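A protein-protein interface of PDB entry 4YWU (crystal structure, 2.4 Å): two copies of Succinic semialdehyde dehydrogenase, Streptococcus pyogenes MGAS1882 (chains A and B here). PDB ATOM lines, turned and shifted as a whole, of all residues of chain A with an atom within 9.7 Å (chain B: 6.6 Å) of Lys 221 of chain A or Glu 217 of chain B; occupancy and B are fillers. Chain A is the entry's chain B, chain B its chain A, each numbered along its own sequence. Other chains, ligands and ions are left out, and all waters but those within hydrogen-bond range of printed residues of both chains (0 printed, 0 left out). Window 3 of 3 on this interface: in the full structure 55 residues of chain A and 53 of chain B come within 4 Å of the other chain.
Ala 213 of chain A touches Gly 220 of chain B, and with the chains exchanged Gly 220 of chain A touches Ala 213 of chain B.
Glu 217 of chain A touches its own counterpart, Glu 217 of chain B.
Glu 217 of chain A touches Gly 220 of chain B, and with the chains exchanged Gly 220 of chain A touches Glu 217 of chain B.
Glu 217 of chain A touches Lys 221 of chain B, and with the chains exchanged Lys 221 of chain A touches Glu 217 of chain B.
Of the 12 pairs that touch across the chains among the printed residues, 11 have their exchanged pair printed and touching as well.
Among the printed residues, pairs that only touch across the chains: Ala 213 of chain A with Gly 220 of chain B (3.6 Å), Ala 213 of chain A with Lys 221 of chain B (3.7 Å), Ala 216 of chain A with Gly 220 of chain B (3.3 Å), Glu 217 of chain A with Glu 217 of chain B (3.6 Å), Glu 217 of chain A with Gly 220 of chain B (3.8 Å), Glu 217 of chain A with Lys 221 of chain B (3.3 Å), Gly 220 of chain A with Ala 216 of chain B (3.2 Å), Gly 220 of chain A with Glu 217 of chain B (3.8 Å), Lys 221 of chain A with Ala 213 of chain B (3.8 Å), Lys 221 of chain A with Glu 217 of chain B (3.4 Å) and Leu 223 of chain A with Ala 213 of chain B (3.7 Å).
Hydrophobic or aromatic side chains of chain A within 4 Å of the printed part of chain B: Ala 213, Ala 216 and Leu 223.
Of the 12 printed residues of chain B, 5 touch a printed residue of chain A.
Among the printed residues, 12 pairs touch across the chains.
Among the printed residues, no Asp or Glu carboxylate lies within 4 Å of a Lys or Arg side-chain nitrogen of the other chain.
O of Gly 220 of chain A lies close to O of Ala 213 of chain B (3.4 Å).
Ile 195 of chain A touches none of the printed residues of chain B.
Val 203 of chain A touches none of the printed residues of chain B.
Printed residues of chain B within 4 Å of Ala 213 of chain A: Gly 220 (3.6 Å) and Lys 221 (3.7 Å).
Of the printed residues of chain B, Ala 216 of chain A touches Gly 220 (3.3 Å).
Printed residues of chain B within 4 Å of Glu 217 of chain A: Glu 217, Gly 220 and Lys 221.
Of chain B, only Ala 213 and Glu 217 come within 4 Å of Lys 221 of chain A.
Of the printed residues of chain A, Ala 213 of chain B touches Gly 220 (3.4 Å), Lys 221 (3.8 Å) and Leu 223 (3.7 Å).
Ala 216 of chain B touches just one residue of chain A: Gly 220 (3.2 Å).
Of chain A, only Glu 217 (3.6 Å), Gly 220 (3.8 Å) and Lys 221 (3.4 Å) come within 4 Å of Glu 217 of chain B.
Gly 220 of chain B touches three residues of chain A.
Of the printed residues of chain A, Lys 221 of chain B touches Ala 213 and Glu 217.
The nearest residue of chain A that does not touch Glu 217 of chain B is Ala 216 of chain A (5.4 Å).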
ATOM      1  N   SER A 192       7.719  14.510 -17.492  1.00  0.00           N
ATOM      2  CA  SER A 192       7.739  13.223 -18.165  1.00  0.00           C
ATOM      3  C   SER A 192       6.493  12.435 -17.803  1.00  0.00           C
ATOM      4  O   SER A 192       6.010  11.641 -18.601  1.00  0.00           O
ATOM      5  CB  SER A 192       8.982  12.432 -17.779  1.00  0.00           C
ATOM      6  OG  SER A 192       8.870  11.952 -16.458  1.00  0.00           O
ATOM      7  N   GLN A 193       5.979  12.644 -16.596  1.00  0.00           N
ATOM      8  CA  GLN A 193       4.761  11.959 -16.154  1.00  0.00           C
ATOM      9  C   GLN A 193       3.566  12.476 -16.959  1.00  0.00           C
ATOM     10  O   GLN A 193       2.708  11.705 -17.397  1.00  0.00           O
ATOM     11  CB  GLN A 193       4.502  12.227 -14.676  1.00  0.00           C
ATOM     12  CG  GLN A 193       5.466  11.561 -13.730  1.00  0.00           C
ATOM     13  CD  GLN A 193       5.246  12.010 -12.295  1.00  0.00           C
ATOM     14  OE1 GLN A 193       4.099  12.132 -11.834  1.00  0.00           O
ATOM     15  NE2 GLN A 193       6.345  12.253 -11.574  1.00  0.00           N
ATOM     16  N   ILE A 195       3.643  13.835 -19.890  1.00  0.00           N
ATOM     17  CA  ILE A 195       3.784  13.316 -21.244  1.00  0.00           C
ATOM     18  C   ILE A 195       3.346  11.850 -21.330  1.00  0.00           C
ATOM     19  O   ILE A 195       2.725  11.436 -22.308  1.00  0.00           O
ATOM     20  CB  ILE A 195       5.249  13.445 -21.735  1.00  0.00           C
ATOM     21  CG1 ILE A 195       5.607  14.923 -21.904  1.00  0.00           C
ATOM     22  CG2 ILE A 195       5.439  12.689 -23.051  1.00  0.00           C
ATOM     23  CD1 ILE A 195       7.072  15.176 -22.237  1.00  0.00           C
ATOM     24  N   ALA A 196       3.660  11.075 -20.302  1.00  0.00           N
ATOM     25  CA  ALA A 196       3.315   9.660 -20.271  1.00  0.00           C
ATOM     26  C   ALA A 196       1.840   9.413 -19.969  1.00  0.00           C
ATOM     27  O   ALA A 196       1.352   8.291 -20.107  1.00  0.00           O
ATOM     28  CB  ALA A 196       4.177   8.944 -19.246  1.00  0.00           C
ATOM     29  N   ASP A 197       1.133  10.457 -19.552  1.00  0.00           N
ATOM     30  CA  ASP A 197      -0.282  10.332 -19.235  1.00  0.00           C
ATOM     31  C   ASP A 197      -1.105  10.184 -20.515  1.00  0.00           C
ATOM     32  O   ASP A 197      -0.955  10.972 -21.446  1.00  0.00           O
ATOM     33  CB  ASP A 197      -0.741  11.554 -18.452  1.00  0.00           C
ATOM     34  CG  ASP A 197      -2.100  11.355 -17.812  1.00  0.00           C
ATOM     35  OD1 ASP A 197      -3.103  11.200 -18.551  1.00  0.00           O
ATOM     36  OD2 ASP A 197      -2.157  11.351 -16.560  1.00  0.00           O
ATOM     37  N   VAL A 203       2.740  17.377 -27.541  1.00  0.00           N
ATOM     38  CA  VAL A 203       3.568  18.350 -26.838  1.00  0.00           C
ATOM     39  C   VAL A 203       4.187  19.348 -27.794  1.00  0.00           C
ATOM     40  O   VAL A 203       4.695  18.969 -28.857  1.00  0.00           O
ATOM     41  CB  VAL A 203       4.747  17.688 -26.095  1.00  0.00           C
ATOM     42  CG1 VAL A 203       5.397  18.713 -25.174  1.00  0.00           C
ATOM     43  CG2 VAL A 203       4.281  16.463 -25.326  1.00  0.00           C
ATOM     44  N   GLY A 212      14.719  20.093 -25.551  1.00  0.00           N
ATOM     45  CA  GLY A 212      13.989  19.599 -26.702  1.00  0.00           C
ATOM     46  C   GLY A 212      14.232  18.120 -26.900  1.00  0.00           C
ATOM     47  O   GLY A 212      13.291  17.354 -27.067  1.00  0.00           O
ATOM     48  N   ALA A 213      15.496  17.717 -26.874  1.00  0.00           N
ATOM     49  CA  ALA A 213      15.847  16.318 -27.057  1.00  0.00           C
ATOM     50  C   ALA A 213      15.224  15.499 -25.946  1.00  0.00           C
ATOM     51  O   ALA A 213      14.620  14.454 -26.186  1.00  0.00           O
ATOM     52  CB  ALA A 213      17.360  16.149 -27.041  1.00  0.00           C
ATOM     53  N   SER A 214      15.367  15.989 -24.722  1.00  0.00           N
ATOM     54  CA  SER A 214      14.832  15.296 -23.562  1.00  0.00           C
ATOM     55  C   SER A 214      13.332  15.051 -23.686  1.00  0.00           C
ATOM     56  O   SER A 214      12.874  13.913 -23.608  1.00  0.00           O
ATOM     57  CB  SER A 214      15.136  16.097 -22.299  1.00  0.00           C
ATOM     58  OG  SER A 214      14.529  15.492 -21.174  1.00  0.00           O
ATOM     59  N   ILE A 215      12.569  16.121 -23.877  1.00  0.00           N
ATOM     60  CA  ILE A 215      11.116  16.017 -24.014  1.00  0.00           C
ATOM     61  C   ILE A 215      10.690  15.222 -25.253  1.00  0.00           C
ATOM     62  O   ILE A 215       9.809  14.361 -25.174  1.00  0.00           O
ATOM     63  CB  ILE A 215      10.460  17.437 -24.054  1.00  0.00           C
ATOM     64  CG1 ILE A 215      10.255  17.960 -22.631  1.00  0.00           C
ATOM     65  CG2 ILE A 215       9.125  17.394 -24.774  1.00  0.00           C
ATOM     66  CD1 ILE A 215      11.524  18.064 -21.816  1.00  0.00           C
ATOM     67  N   ALA A 216      11.305  15.508 -26.393  1.00  0.00           N
ATOM     68  CA  ALA A 216      10.959  14.811 -27.629  1.00  0.00           C
ATOM     69  C   ALA A 216      11.076  13.301 -27.448  1.00  0.00           C
ATOM     70  O   ALA A 216      10.223  12.534 -27.901  1.00  0.00           O
ATOM     71  CB  ALA A 216      11.863  15.279 -28.769  1.00  0.00           C
ATOM     72  N   GLU A 217      12.143  12.888 -26.776  1.00  0.00           N
ATOM     73  CA  GLU A 217      12.403  11.480 -26.521  1.00  0.00           C
ATOM     74  C   GLU A 217      11.292  10.861 -25.676  1.00  0.00           C
ATOM     75  O   GLU A 217      10.774   9.802 -26.011  1.00  0.00           O
ATOM     76  CB  GLU A 217      13.748  11.339 -25.818  1.00  0.00           C
ATOM     77  CG  GLU A 217      14.158   9.922 -25.543  1.00  0.00           C
ATOM     78  CD  GLU A 217      15.491   9.842 -24.824  1.00  0.00           C
ATOM     79  OE1 GLU A 217      15.606  10.426 -23.726  1.00  0.00           O
ATOM     80  OE2 GLU A 217      16.422   9.196 -25.354  1.00  0.00           O
ATOM     81  N   GLU A 218      10.923  11.523 -24.582  1.00  0.00           N
ATOM     82  CA  GLU A 218       9.861  11.026 -23.717  1.00  0.00           C
ATOM     83  C   GLU A 218       8.568  11.019 -24.521  1.00  0.00           C
ATOM     84  O   GLU A 218       7.738  10.120 -24.389  1.00  0.00           O
ATOM     85  CB  GLU A 218       9.697  11.935 -22.496  1.00  0.00           C
ATOM     86  CG  GLU A 218      11.001  12.221 -21.757  1.00  0.00           C
ATOM     87  CD  GLU A 218      10.844  13.222 -20.604  1.00  0.00           C
ATOM     88  OE1 GLU A 218      10.084  14.207 -20.759  1.00  0.00           O
ATOM     89  OE2 GLU A 218      11.500  13.034 -19.549  1.00  0.00           O
ATOM     90  N   ALA A 219       8.399  12.033 -25.360  1.00  0.00           N
ATOM     91  CA  ALA A 219       7.201  12.134 -26.176  1.00  0.00           C
ATOM     92  C   ALA A 219       7.113  10.961 -27.139  1.00  0.00           C
ATOM     93  O   ALA A 219       6.059  10.348 -27.289  1.00  0.00           O
ATOM     94  CB  ALA A 219       7.208  13.442 -26.949  1.00  0.00           C
ATOM     95  N   GLY A 220       8.233  10.658 -27.787  1.00  0.00           N
ATOM     96  CA  GLY A 220       8.278   9.567 -28.744  1.00  0.00           C
ATOM     97  C   GLY A 220       8.116   8.196 -28.120  1.00  0.00           C
ATOM     98  O   GLY A 220       7.629   7.260 -28.765  1.00  0.00           O
ATOM     99  N   LYS A 221       8.535   8.077 -26.865  1.00  0.00           N
ATOM    100  CA  LYS A 221       8.413   6.824 -26.132  1.00  0.00           C
ATOM    101  C   LYS A 221       6.950   6.546 -25.820  1.00  0.00           C
ATOM    102  O   LYS A 221       6.562   5.401 -25.587  1.00  0.00           O
ATOM    103  CB  LYS A 221       9.228   6.878 -24.838  1.00  0.00           C
ATOM    104  CG  LYS A 221       8.866   5.797 -23.833  1.00  0.00           C
ATOM    105  CD  LYS A 221       9.962   5.618 -22.795  1.00  0.00           C
ATOM    106  CE  LYS A 221       9.415   5.015 -21.512  1.00  0.00           C
ATOM    107  NZ  LYS A 221       8.912   6.060 -20.578  1.00  0.00           N
ATOM    108  N   ASN A 222       6.140   7.600 -25.821  1.00  0.00           N
ATOM    109  CA  ASN A 222       4.717   7.458 -25.566  1.00  0.00           C
ATOM    110  C   ASN A 222       3.853   7.819 -26.768  1.00  0.00           C
ATOM    111  O   ASN A 222       2.712   8.259 -26.610  1.00  0.00           O
ATOM    112  CB  ASN A 222       4.307   8.298 -24.351  1.00  0.00           C
ATOM    113  CG  ASN A 222       4.990   7.844 -23.065  1.00  0.00           C
ATOM    114  OD1 ASN A 222       6.078   8.315 -22.716  1.00  0.00           O
ATOM    115  ND2 ASN A 222       4.355   6.913 -22.361  1.00  0.00           N
ATOM    116  N   LEU A 223       4.405   7.629 -27.965  1.00  0.00           N
ATOM    117  CA  LEU A 223       3.693   7.891 -29.213  1.00  0.00           C
ATOM    118  C   LEU A 223       2.950   9.227 -29.292  1.00  0.00           C
ATOM    119  O   LEU A 223       1.902   9.311 -29.941  1.00  0.00           O
ATOM    120  CB  LEU A 223       2.686   6.778 -29.464  1.00  0.00           C
ATOM    121  CG  LEU A 223       3.099   5.368 -29.048  1.00  0.00           C
ATOM    122  CD1 LEU A 223       1.964   4.425 -29.418  1.00  0.00           C
ATOM    123  CD2 LEU A 223       4.401   4.949 -29.734  1.00  0.00           C
ATOM    124  N   LYS A 224       3.481  10.261 -28.645  1.00  0.00           N
ATOM    125  CA  LYS A 224       2.844  11.571 -28.669  1.00  0.00           C
ATOM    126  C   LYS A 224       3.472  12.460 -29.737  1.00  0.00           C
ATOM    127  O   LYS A 224       4.693  12.488 -29.893  1.00  0.00           O
ATOM    128  CB  LYS A 224       2.985  12.244 -27.305  1.00  0.00           C
ATOM    129  CG  LYS A 224       2.470  11.417 -26.137  1.00  0.00           C
ATOM    130  CD  LYS A 224       0.978  11.174 -26.230  1.00  0.00           C
ATOM    131  CE  LYS A 224       0.508  10.173 -25.174  1.00  0.00           C
ATOM    132  NZ  LYS A 224       0.677  10.650 -23.767  1.00  0.00           N
ATOM    133  N   LYS A 225       2.635  13.186 -30.471  1.00  0.00           N
ATOM    134  CA  LYS A 225       3.117  14.090 -31.511  1.00  0.00           C
ATOM    135  C   LYS A 225       3.766  15.312 -30.878  1.00  0.00           C
ATOM    136  O   LYS A 225       3.336  15.776 -29.818  1.00  0.00           O
ATOM    137  CB  LYS A 225       1.956  14.545 -32.398  1.00  0.00           C
ATOM    138  CG  LYS A 225       2.347  15.487 -33.525  1.00  0.00           C
ATOM    139  CD  LYS A 225       1.177  15.718 -34.474  1.00  0.00           C
ATOM    140  CE  LYS A 225       1.552  16.659 -35.611  1.00  0.00           C
ATOM    141  NZ  LYS A 225       0.490  16.694 -36.662  1.00  0.00           N
ATOM    142  N   THR A 226       4.793  15.843 -31.534  1.00  0.00           N
ATOM    143  CA  THR A 226       5.484  17.019 -31.020  1.00  0.00           C
ATOM    144  C   THR A 226       5.812  18.041 -32.100  1.00  0.00           C
ATOM    145  O   THR A 226       5.646  17.793 -33.286  1.00  0.00           O
ATOM    146  CB  THR A 226       6.821  16.636 -30.356  1.00  0.00           C
ATOM    147  OG1 THR A 226       7.658  16.007 -31.329  1.00  0.00           O
ATOM    148  CG2 THR A 226       6.607  15.687 -29.194  1.00  0.00           C
ATOM    149  N   TYR A 434      11.410  21.497 -35.682  1.00  0.00           N
ATOM    150  CA  TYR A 434      10.521  21.105 -36.776  1.00  0.00           C
ATOM    151  C   TYR A 434       9.085  21.438 -36.390  1.00  0.00           C
ATOM    152  O   TYR A 434       8.746  21.491 -35.205  1.00  0.00           O
ATOM    153  CB  TYR A 434      10.664  19.609 -37.105  1.00  0.00           C
ATOM    154  CG  TYR A 434      10.515  18.676 -35.926  1.00  0.00           C
ATOM    155  CD1 TYR A 434       9.260  18.384 -35.391  1.00  0.00           C
ATOM    156  CD2 TYR A 434      11.637  18.097 -35.332  1.00  0.00           C
ATOM    157  CE1 TYR A 434       9.126  17.543 -34.288  1.00  0.00           C
ATOM    158  CE2 TYR A 434      11.517  17.252 -34.238  1.00  0.00           C
ATOM    159  CZ  TYR A 434      10.261  16.981 -33.718  1.00  0.00           C
ATOM    160  OH  TYR A 434      10.151  16.161 -32.620  1.00  0.00           O
ATOM    161  N   GLY B 211       7.698  -1.266 -31.878  1.00  0.00           N
ATOM    162  CA  GLY B 211       8.682  -0.719 -32.791  1.00  0.00           C
ATOM    163  C   GLY B 211       8.578   0.789 -32.889  1.00  0.00           C
ATOM    164  O   GLY B 211       9.586   1.493 -32.830  1.00  0.00           O
ATOM    165  N   GLY B 212       7.354   1.287 -33.037  1.00  0.00           N
ATOM    166  CA  GLY B 212       7.143   2.719 -33.142  1.00  0.00           C
ATOM    167  C   GLY B 212       7.662   3.480 -31.938  1.00  0.00           C
ATOM    168  O   GLY B 212       8.327   4.508 -32.085  1.00  0.00           O
ATOM    169  N   ALA B 213       7.368   2.984 -30.741  1.00  0.00           N
ATOM    170  CA  ALA B 213       7.822   3.652 -29.526  1.00  0.00           C
ATOM    171  C   ALA B 213       9.344   3.733 -29.529  1.00  0.00           C
ATOM    172  O   ALA B 213       9.926   4.789 -29.282  1.00  0.00           O
ATOM    173  CB  ALA B 213       7.336   2.896 -28.303  1.00  0.00           C
ATOM    174  N   SER B 214       9.981   2.607 -29.822  1.00  0.00           N
ATOM    175  CA  SER B 214      11.435   2.522 -29.879  1.00  0.00           C
ATOM    176  C   SER B 214      11.997   3.503 -30.917  1.00  0.00           C
ATOM    177  O   SER B 214      12.879   4.302 -30.628  1.00  0.00           O
ATOM    178  CB  SER B 214      11.831   1.071 -30.211  1.00  0.00           C
ATOM    179  OG  SER B 214      13.186   0.946 -30.624  1.00  0.00           O
ATOM    180  N   ILE B 215      11.468   3.450 -32.126  1.00  0.00           N
ATOM    181  CA  ILE B 215      11.933   4.322 -33.191  1.00  0.00           C
ATOM    182  C   ILE B 215      11.648   5.807 -32.916  1.00  0.00           C
ATOM    183  O   ILE B 215      12.511   6.662 -33.148  1.00  0.00           O
ATOM    184  CB  ILE B 215      11.308   3.897 -34.533  1.00  0.00           C
ATOM    185  CG1 ILE B 215      11.591   2.411 -34.787  1.00  0.00           C
ATOM    186  CG2 ILE B 215      11.878   4.737 -35.672  1.00  0.00           C
ATOM    187  CD1 ILE B 215      13.050   2.060 -34.930  1.00  0.00           C
ATOM    188  N   ALA B 216      10.450   6.117 -32.420  1.00  0.00           N
ATOM    189  CA  ALA B 216      10.102   7.509 -32.116  1.00  0.00           C
ATOM    190  C   ALA B 216      10.976   8.017 -30.970  1.00  0.00           C
ATOM    191  O   ALA B 216      11.373   9.176 -30.937  1.00  0.00           O
ATOM    192  CB  ALA B 216       8.630   7.625 -31.744  1.00  0.00           C
ATOM    193  N   GLU B 217      11.285   7.141 -30.028  1.00  0.00           N
ATOM    194  CA  GLU B 217      12.120   7.536 -28.916  1.00  0.00           C
ATOM    195  C   GLU B 217      13.513   7.943 -29.407  1.00  0.00           C
ATOM    196  O   GLU B 217      14.063   8.952 -28.972  1.00  0.00           O
ATOM    197  CB  GLU B 217      12.217   6.386 -27.921  1.00  0.00           C
ATOM    198  CG  GLU B 217      13.107   6.681 -26.737  1.00  0.00           C
ATOM    199  CD  GLU B 217      12.952   5.659 -25.632  1.00  0.00           C
ATOM    200  OE1 GLU B 217      12.922   4.446 -25.946  1.00  0.00           O
ATOM    201  OE2 GLU B 217      12.872   6.067 -24.449  1.00  0.00           O
ATOM    202  N   GLU B 218      14.076   7.167 -30.326  1.00  0.00           N
ATOM    203  CA  GLU B 218      15.402   7.464 -30.854  1.00  0.00           C
ATOM    204  C   GLU B 218      15.345   8.698 -31.727  1.00  0.00           C
ATOM    205  O   GLU B 218      16.268   9.507 -31.727  1.00  0.00           O
ATOM    206  CB  GLU B 218      15.934   6.272 -31.659  1.00  0.00           C
ATOM    207  CG  GLU B 218      15.882   4.965 -30.866  1.00  0.00           C
ATOM    208  CD  GLU B 218      16.339   3.741 -31.654  1.00  0.00           C
ATOM    209  OE1 GLU B 218      15.961   3.605 -32.843  1.00  0.00           O
ATOM    210  OE2 GLU B 218      17.061   2.901 -31.066  1.00  0.00           O
ATOM    211  N   ALA B 219      14.256   8.850 -32.468  1.00  0.00           N
ATOM    212  CA  ALA B 219      14.113  10.008 -33.341  1.00  0.00           C
ATOM    213  C   ALA B 219      14.012  11.277 -32.500  1.00  0.00           C
ATOM    214  O   ALA B 219      14.579  12.308 -32.848  1.00  0.00           O
ATOM    215  CB  ALA B 219      12.875   9.856 -34.231  1.00  0.00           C
ATOM    216  N   GLY B 220      13.290  11.190 -31.388  1.00  0.00           N
ATOM    217  CA  GLY B 220      13.131  12.340 -30.522  1.00  0.00           C
ATOM    218  C   GLY B 220      14.428  12.738 -29.853  1.00  0.00           C
ATOM    219  O   GLY B 220      14.731  13.922 -29.722  1.00  0.00           O
ATOM    220  N   LYS B 221      15.202  11.750 -29.422  1.00  0.00           N
ATOM    221  CA  LYS B 221      16.471  12.027 -28.759  1.00  0.00           C
ATOM    222  C   LYS B 221      17.424  12.737 -29.715  1.00  0.00           C
ATOM    223  O   LYS B 221      18.392  13.367 -29.284  1.00  0.00           O
ATOM    224  CB  LYS B 221      17.106  10.721 -28.261  1.00  0.00           C
ATOM    225  CG  LYS B 221      18.540  10.864 -27.763  1.00  0.00           C
ATOM    226  CD  LYS B 221      19.113   9.535 -27.291  1.00  0.00           C
ATOM    227  CE  LYS B 221      19.159   8.510 -28.424  1.00  0.00           C
ATOM    228  NZ  LYS B 221      19.666   7.179 -27.973  1.00  0.00           N
ATOM    229  N   ASN B 222      17.132  12.647 -31.010  1.00  0.00           N
ATOM    230  CA  ASN B 222      17.971  13.258 -32.030  1.00  0.00           C
ATOM    231  C   ASN B 222      17.301  14.381 -32.798  1.00  0.00           C
ATOM    232  O   ASN B 222      17.777  14.771 -33.864  1.00  0.00           O
ATOM    233  CB  ASN B 222      18.437  12.182 -32.999  1.00  0.00           C
ATOM    234  CG  ASN B 222      19.352  11.183 -32.336  1.00  0.00           C
ATOM    235  OD1 ASN B 222      20.525  11.467 -32.102  1.00  0.00           O
ATOM    236  ND2 ASN B 222      18.816  10.011 -32.004  1.00  0.00           N
